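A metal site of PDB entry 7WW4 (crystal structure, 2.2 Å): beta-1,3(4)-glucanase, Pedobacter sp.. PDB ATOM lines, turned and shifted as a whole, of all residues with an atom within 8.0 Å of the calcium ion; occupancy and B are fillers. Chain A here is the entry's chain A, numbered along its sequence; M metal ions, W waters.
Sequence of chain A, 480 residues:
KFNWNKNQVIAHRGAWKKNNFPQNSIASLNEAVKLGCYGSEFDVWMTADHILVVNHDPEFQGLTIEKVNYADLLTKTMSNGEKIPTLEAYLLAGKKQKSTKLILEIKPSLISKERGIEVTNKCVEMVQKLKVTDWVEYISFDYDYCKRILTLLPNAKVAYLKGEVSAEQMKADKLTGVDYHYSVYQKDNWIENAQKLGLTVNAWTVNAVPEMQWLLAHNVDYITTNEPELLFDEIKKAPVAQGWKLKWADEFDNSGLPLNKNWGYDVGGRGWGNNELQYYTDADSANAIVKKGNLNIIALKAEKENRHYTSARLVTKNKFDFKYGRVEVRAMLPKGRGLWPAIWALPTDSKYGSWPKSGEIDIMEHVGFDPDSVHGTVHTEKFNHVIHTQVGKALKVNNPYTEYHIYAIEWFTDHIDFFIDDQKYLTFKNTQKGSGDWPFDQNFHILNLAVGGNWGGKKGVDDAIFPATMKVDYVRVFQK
Merely in contact with the calcium ion: Asp 253 (3.98 Å).
Within 4 Å of the calcium ion: Glu 251, Asp 253, Gly 293 and Asp 473.
The backbone carbonyl oxygen (O) of Glu 251 binds the calcium ion (2.5 Å).
Water W1 is bound to the calcium ion (2.5 Å).
The backbone carbonyl oxygen (O) of Gly 293 binds the calcium ion (2.7 Å).
OD1 of Asp 473 is bound to the calcium ion (2.7 Å).
Slightly farther from the calcium ion lies the backbone carbonyl oxygen (O) of Asp 473 (3.1 Å).
The guanidinium group (NH1) of Arg 330 lies within salt-bridge range of the side-chain carboxylate (OD2) of Asp 473 (2.4 Å).
OE1 of Glu 251 lies within salt-bridge range of NE of Arg 476.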
ATOM      1  N   GLN A 186      13.028  -1.970  27.959  1.00  0.00           N
ATOM      2  CA  GLN A 186      11.623  -1.732  27.705  1.00  0.00           C
ATOM      3  C   GLN A 186      11.434  -0.574  26.727  1.00  0.00           C
ATOM      4  O   GLN A 186      10.692   0.377  27.007  1.00  0.00           O
ATOM      5  CB  GLN A 186      10.875  -1.463  29.020  1.00  0.00           C
ATOM      6  CG  GLN A 186      10.881  -2.664  29.960  1.00  0.00           C
ATOM      7  CD  GLN A 186      10.494  -2.302  31.380  1.00  0.00           C
ATOM      8  OE1 GLN A 186      10.442  -1.128  31.744  1.00  0.00           O
ATOM      9  NE2 GLN A 186      10.227  -3.319  32.189  1.00  0.00           N
ATOM     10  N   TRP A 214       8.940 -12.190  30.385  1.00  0.00           N
ATOM     11  CA  TRP A 214       9.061 -11.175  29.341  1.00  0.00           C
ATOM     12  C   TRP A 214      10.417 -11.269  28.643  1.00  0.00           C
ATOM     13  O   TRP A 214      10.498 -11.098  27.422  1.00  0.00           O
ATOM     14  CB  TRP A 214       8.850  -9.785  29.932  1.00  0.00           C
ATOM     15  CG  TRP A 214       9.369  -8.680  29.073  1.00  0.00           C
ATOM     16  CD1 TRP A 214       8.928  -8.322  27.826  1.00  0.00           C
ATOM     17  CD2 TRP A 214      10.432  -7.772  29.389  1.00  0.00           C
ATOM     18  NE1 TRP A 214       9.649  -7.257  27.358  1.00  0.00           N
ATOM     19  CE2 TRP A 214      10.577  -6.897  28.293  1.00  0.00           C
ATOM     20  CE3 TRP A 214      11.271  -7.606  30.499  1.00  0.00           C
ATOM     21  CZ2 TRP A 214      11.528  -5.879  28.274  1.00  0.00           C
ATOM     22  CZ3 TRP A 214      12.215  -6.597  30.481  1.00  0.00           C
ATOM     23  CH2 TRP A 214      12.336  -5.740  29.373  1.00  0.00           C
ATOM     24  N   ASP A 250       3.236  -6.761  21.843  1.00  0.00           N
ATOM     25  CA  ASP A 250       3.133  -5.386  22.324  1.00  0.00           C
ATOM     26  C   ASP A 250       3.128  -5.429  23.847  1.00  0.00           C
ATOM     27  O   ASP A 250       2.136  -5.848  24.457  1.00  0.00           O
ATOM     28  CB  ASP A 250       1.877  -4.693  21.794  1.00  0.00           C
ATOM     29  CG  ASP A 250       1.865  -3.192  22.050  1.00  0.00           C
ATOM     30  OD1 ASP A 250       2.731  -2.708  22.803  1.00  0.00           O
ATOM     31  OD2 ASP A 250       0.988  -2.504  21.503  1.00  0.00           O
ATOM     32  N   GLU A 251       4.232  -5.016  24.453  1.00  0.00           N
ATOM     33  CA  GLU A 251       4.369  -4.998  25.909  1.00  0.00           C
ATOM     34  C   GLU A 251       3.853  -3.704  26.531  1.00  0.00           C
ATOM     35  O   GLU A 251       3.866  -3.589  27.767  1.00  0.00           O
ATOM     36  CB  GLU A 251       5.827  -5.224  26.306  1.00  0.00           C
ATOM     37  CG  GLU A 251       6.504  -6.369  25.542  1.00  0.00           C
ATOM     38  CD  GLU A 251       6.077  -7.731  26.043  1.00  0.00           C
ATOM     39  OE1 GLU A 251       5.991  -8.672  25.212  1.00  0.00           O
ATOM     40  OE2 GLU A 251       5.821  -7.873  27.255  1.00  0.00           O
ATOM     41  N   PHE A 252       3.426  -2.747  25.720  1.00  0.00           N
ATOM     42  CA  PHE A 252       2.772  -1.526  26.184  1.00  0.00           C
ATOM     43  C   PHE A 252       3.699  -0.673  27.054  1.00  0.00           C
ATOM     44  O   PHE A 252       3.290  -0.108  28.066  1.00  0.00           O
ATOM     45  CB  PHE A 252       1.476  -1.845  26.932  1.00  0.00           C
ATOM     46  CG  PHE A 252       0.422  -2.475  26.066  1.00  0.00           C
ATOM     47  CD1 PHE A 252       0.066  -1.901  24.856  1.00  0.00           C
ATOM     48  CD2 PHE A 252      -0.207  -3.646  26.448  1.00  0.00           C
ATOM     49  CE1 PHE A 252      -0.897  -2.476  24.049  1.00  0.00           C
ATOM     50  CE2 PHE A 252      -1.176  -4.228  25.642  1.00  0.00           C
ATOM     51  CZ  PHE A 252      -1.516  -3.641  24.453  1.00  0.00           C
ATOM     52  N   ASP A 253       4.953  -0.570  26.640  1.00  0.00           N
ATOM     53  CA  ASP A 253       5.844   0.461  27.157  1.00  0.00           C
ATOM     54  C   ASP A 253       5.682   1.784  26.411  1.00  0.00           C
ATOM     55  O   ASP A 253       6.536   2.665  26.534  1.00  0.00           O
ATOM     56  CB  ASP A 253       7.304  -0.002  27.080  1.00  0.00           C
ATOM     57  CG  ASP A 253       7.494  -1.436  27.532  1.00  0.00           C
ATOM     58  OD1 ASP A 253       8.202  -2.188  26.833  1.00  0.00           O
ATOM     59  OD2 ASP A 253       6.938  -1.802  28.582  1.00  0.00           O
ATOM     60  N   ASN A 254       4.594   1.926  25.648  1.00  0.00           N
ATOM     61  CA  ASN A 254       4.455   3.031  24.710  1.00  0.00           C
ATOM     62  C   ASN A 254       4.229   4.358  25.424  1.00  0.00           C
ATOM     63  O   ASN A 254       4.701   5.397  24.953  1.00  0.00           O
ATOM     64  CB  ASN A 254       3.319   2.725  23.733  1.00  0.00           C
ATOM     65  CG  ASN A 254       2.703   3.976  23.150  1.00  0.00           C
ATOM     66  OD1 ASN A 254       1.603   4.369  23.519  1.00  0.00           O
ATOM     67  N   VAL A 290      -2.168   4.179  27.268  1.00  0.00           N
ATOM     68  CA  VAL A 290      -1.071   3.343  27.722  1.00  0.00           C
ATOM     69  C   VAL A 290      -0.296   4.134  28.760  1.00  0.00           C
ATOM     70  O   VAL A 290       0.325   5.156  28.436  1.00  0.00           O
ATOM     71  CB  VAL A 290      -0.164   2.907  26.554  1.00  0.00           C
ATOM     72  CG1 VAL A 290       0.892   1.924  27.049  1.00  0.00           C
ATOM     73  CG2 VAL A 290      -0.995   2.292  25.439  1.00  0.00           C
ATOM     74  N   LYS A 292       2.192   3.573  32.447  1.00  0.00           N
ATOM     75  CA  LYS A 292       2.869   2.765  33.465  1.00  0.00           C
ATOM     76  C   LYS A 292       3.003   1.300  33.029  1.00  0.00           C
ATOM     77  O   LYS A 292       2.870   0.380  33.836  1.00  0.00           O
ATOM     78  CB  LYS A 292       2.162   2.872  34.819  1.00  0.00           C
ATOM     79  CG  LYS A 292       1.921   4.308  35.261  1.00  0.00           C
ATOM     80  CD  LYS A 292       1.162   4.365  36.572  1.00  0.00           C
ATOM     81  CE  LYS A 292       0.871   5.803  36.972  1.00  0.00           C
ATOM     82  NZ  LYS A 292       0.293   5.894  38.344  1.00  0.00           N
ATOM     83  N   GLY A 293       3.255   1.093  31.739  1.00  0.00           N
ATOM     84  CA  GLY A 293       3.553  -0.224  31.224  1.00  0.00           C
ATOM     85  C   GLY A 293       2.356  -1.110  30.919  1.00  0.00           C
ATOM     86  O   GLY A 293       2.553  -2.273  30.551  1.00  0.00           O
ATOM     87  N   ASN A 294       1.140  -0.601  31.056  1.00  0.00           N
ATOM     88  CA  ASN A 294      -0.065  -1.388  30.813  1.00  0.00           C
ATOM     89  C   ASN A 294      -1.045  -0.597  29.966  1.00  0.00           C
ATOM     90  O   ASN A 294      -1.242   0.602  30.192  1.00  0.00           O
ATOM     91  CB  ASN A 294      -0.735  -1.808  32.131  1.00  0.00           C
ATOM     92  CG  ASN A 294       0.113  -2.778  32.935  1.00  0.00           C
ATOM     93  N   LEU A 295      -1.651  -1.265  28.999  1.00  0.00           N
ATOM     94  CA  LEU A 295      -2.738  -0.668  28.231  1.00  0.00           C
ATOM     95  C   LEU A 295      -3.982  -0.558  29.104  1.00  0.00           C
ATOM     96  O   LEU A 295      -4.320  -1.478  29.848  1.00  0.00           O
ATOM     97  CB  LEU A 295      -3.038  -1.496  26.983  1.00  0.00           C
ATOM     98  CG  LEU A 295      -4.392  -1.246  26.312  1.00  0.00           C
ATOM     99  CD1 LEU A 295      -4.399   0.106  25.612  1.00  0.00           C
ATOM    100  CD2 LEU A 295      -4.746  -2.359  25.347  1.00  0.00           C
ATOM    101  N   ARG A 330      -1.987 -11.005  29.070  1.00  0.00           N
ATOM    102  CA  ARG A 330      -2.004 -10.884  30.517  1.00  0.00           C
ATOM    103  C   ARG A 330      -2.789  -9.621  30.883  1.00  0.00           C
ATOM    104  O   ARG A 330      -2.400  -8.512  30.507  1.00  0.00           O
ATOM    105  CB  ARG A 330      -0.586 -10.812  31.076  1.00  0.00           C
ATOM    106  CG  ARG A 330      -0.492 -10.756  32.589  1.00  0.00           C
ATOM    107  CD  ARG A 330       0.930 -11.081  33.049  1.00  0.00           C
ATOM    108  NE  ARG A 330       1.080 -10.983  34.502  1.00  0.00           N
ATOM    109  CZ  ARG A 330       1.695  -9.980  35.126  1.00  0.00           C
ATOM    110  NH1 ARG A 330       2.219  -8.979  34.423  1.00  0.00           N
ATOM    111  NH2 ARG A 330       1.786  -9.966  36.438  1.00  0.00           N
ATOM    112  N   TYR A 404      -3.142  -9.724  37.995  1.00  0.00           N
ATOM    113  CA  TYR A 404      -3.123 -10.118  36.591  1.00  0.00           C
ATOM    114  C   TYR A 404      -3.245 -11.622  36.443  1.00  0.00           C
ATOM    115  O   TYR A 404      -2.763 -12.402  37.282  1.00  0.00           O
ATOM    116  CB  TYR A 404      -1.836  -9.634  35.912  1.00  0.00           C
ATOM    117  CG  TYR A 404      -1.693  -8.128  35.856  1.00  0.00           C
ATOM    118  CD1 TYR A 404      -1.090  -7.429  36.899  1.00  0.00           C
ATOM    119  CD2 TYR A 404      -2.158  -7.407  34.762  1.00  0.00           C
ATOM    120  CE1 TYR A 404      -0.961  -6.054  36.845  1.00  0.00           C
ATOM    121  CE2 TYR A 404      -2.028  -6.034  34.698  1.00  0.00           C
ATOM    122  CZ  TYR A 404      -1.422  -5.363  35.747  1.00  0.00           C
ATOM    123  OH  TYR A 404      -1.286  -3.994  35.695  1.00  0.00           O
ATOM    124  N   VAL A 472      -4.306  -4.322  30.517  1.00  0.00           N
ATOM    125  CA  VAL A 472      -3.647  -5.398  29.809  1.00  0.00           C
ATOM    126  C   VAL A 472      -2.149  -5.172  29.898  1.00  0.00           C
ATOM    127  O   VAL A 472      -1.635  -4.156  29.408  1.00  0.00           O
ATOM    128  CB  VAL A 472      -4.107  -5.486  28.344  1.00  0.00           C
ATOM    129  CG1 VAL A 472      -3.252  -6.480  27.576  1.00  0.00           C
ATOM    130  CG2 VAL A 472      -5.575  -5.880  28.274  1.00  0.00           C
ATOM    131  N   ASP A 473      -1.429  -6.118  30.515  1.00  0.00           N
ATOM    132  CA  ASP A 473       0.015  -5.989  30.643  1.00  0.00           C
ATOM    133  C   ASP A 473       0.679  -6.073  29.276  1.00  0.00           C
ATOM    134  O   ASP A 473       1.539  -5.237  28.942  1.00  0.00           O
ATOM    135  CB  ASP A 473       0.558  -7.078  31.575  1.00  0.00           C
ATOM    136  CG  ASP A 473       2.050  -6.933  31.833  1.00  0.00           C
ATOM    137  OD1 ASP A 473       2.605  -5.855  31.558  1.00  0.00           O
ATOM    138  OD2 ASP A 473       2.661  -7.910  32.310  1.00  0.00           O
ATOM    139  N   TYR A 474       0.304  -7.060  28.469  1.00  0.00           N
ATOM    140  CA  TYR A 474       0.940  -7.261  27.171  1.00  0.00           C
ATOM    141  C   TYR A 474       0.035  -8.133  26.309  1.00  0.00           C
ATOM    142  O   TYR A 474      -0.902  -8.771  26.786  1.00  0.00           O
ATOM    143  CB  TYR A 474       2.324  -7.902  27.312  1.00  0.00           C
ATOM    144  CG  TYR A 474       2.314  -9.254  27.987  1.00  0.00           C
ATOM    145  CD1 TYR A 474       1.952 -10.403  27.298  1.00  0.00           C
ATOM    146  CD2 TYR A 474       2.676  -9.387  29.331  1.00  0.00           C
ATOM    147  CE1 TYR A 474       1.940 -11.638  27.909  1.00  0.00           C
ATOM    148  CE2 TYR A 474       2.671 -10.628  29.945  1.00  0.00           C
ATOM    149  CZ  TYR A 474       2.304 -11.748  29.227  1.00  0.00           C
ATOM    150  OH  TYR A 474       2.291 -12.983  29.838  1.00  0.00           O
ATOM    151  N   VAL A 475       0.339  -8.150  25.013  1.00  0.00           N
ATOM    152  CA  VAL A 475      -0.254  -9.076  24.058  1.00  0.00           C
ATOM    153  C   VAL A 475       0.877  -9.702  23.252  1.00  0.00           C
ATOM    154  O   VAL A 475       1.589  -8.988  22.529  1.00  0.00           O
ATOM    155  CB  VAL A 475      -1.264  -8.392  23.122  1.00  0.00           C
ATOM    156  CG1 VAL A 475      -1.818  -9.391  22.116  1.00  0.00           C
ATOM    157  CG2 VAL A 475      -2.396  -7.752  23.924  1.00  0.00           C
ATOM    158  N   ARG A 476       1.066 -11.013  23.389  1.00  0.00           N
ATOM    159  CA  ARG A 476       2.133 -11.726  22.712  1.00  0.00           C
ATOM    160  C   ARG A 476       1.556 -12.844  21.870  1.00  0.00           C
ATOM    161  O   ARG A 476       0.601 -13.522  22.268  1.00  0.00           O
ATOM    162  CB  ARG A 476       3.139 -12.301  23.720  1.00  0.00           C
ATOM    163  CG  ARG A 476       3.850 -11.255  24.551  1.00  0.00           C
ATOM    164  CD  ARG A 476       5.022 -11.844  25.324  1.00  0.00           C
ATOM    165  NE  ARG A 476       5.422 -11.000  26.444  1.00  0.00           N
ATOM    166  CZ  ARG A 476       5.436 -11.392  27.716  1.00  0.00           C
ATOM    167  NH1 ARG A 476       5.058 -12.630  28.027  1.00  0.00           N
ATOM    168  NH2 ARG A 476       5.815 -10.548  28.666  1.00  0.00           N
HETATM  169 CA    CA M   1       4.252  -4.299  30.120  1.00  0.00          CA
HETATM  170  O   HOH W   1       5.605  -6.326  29.569  1.00  0.00           O
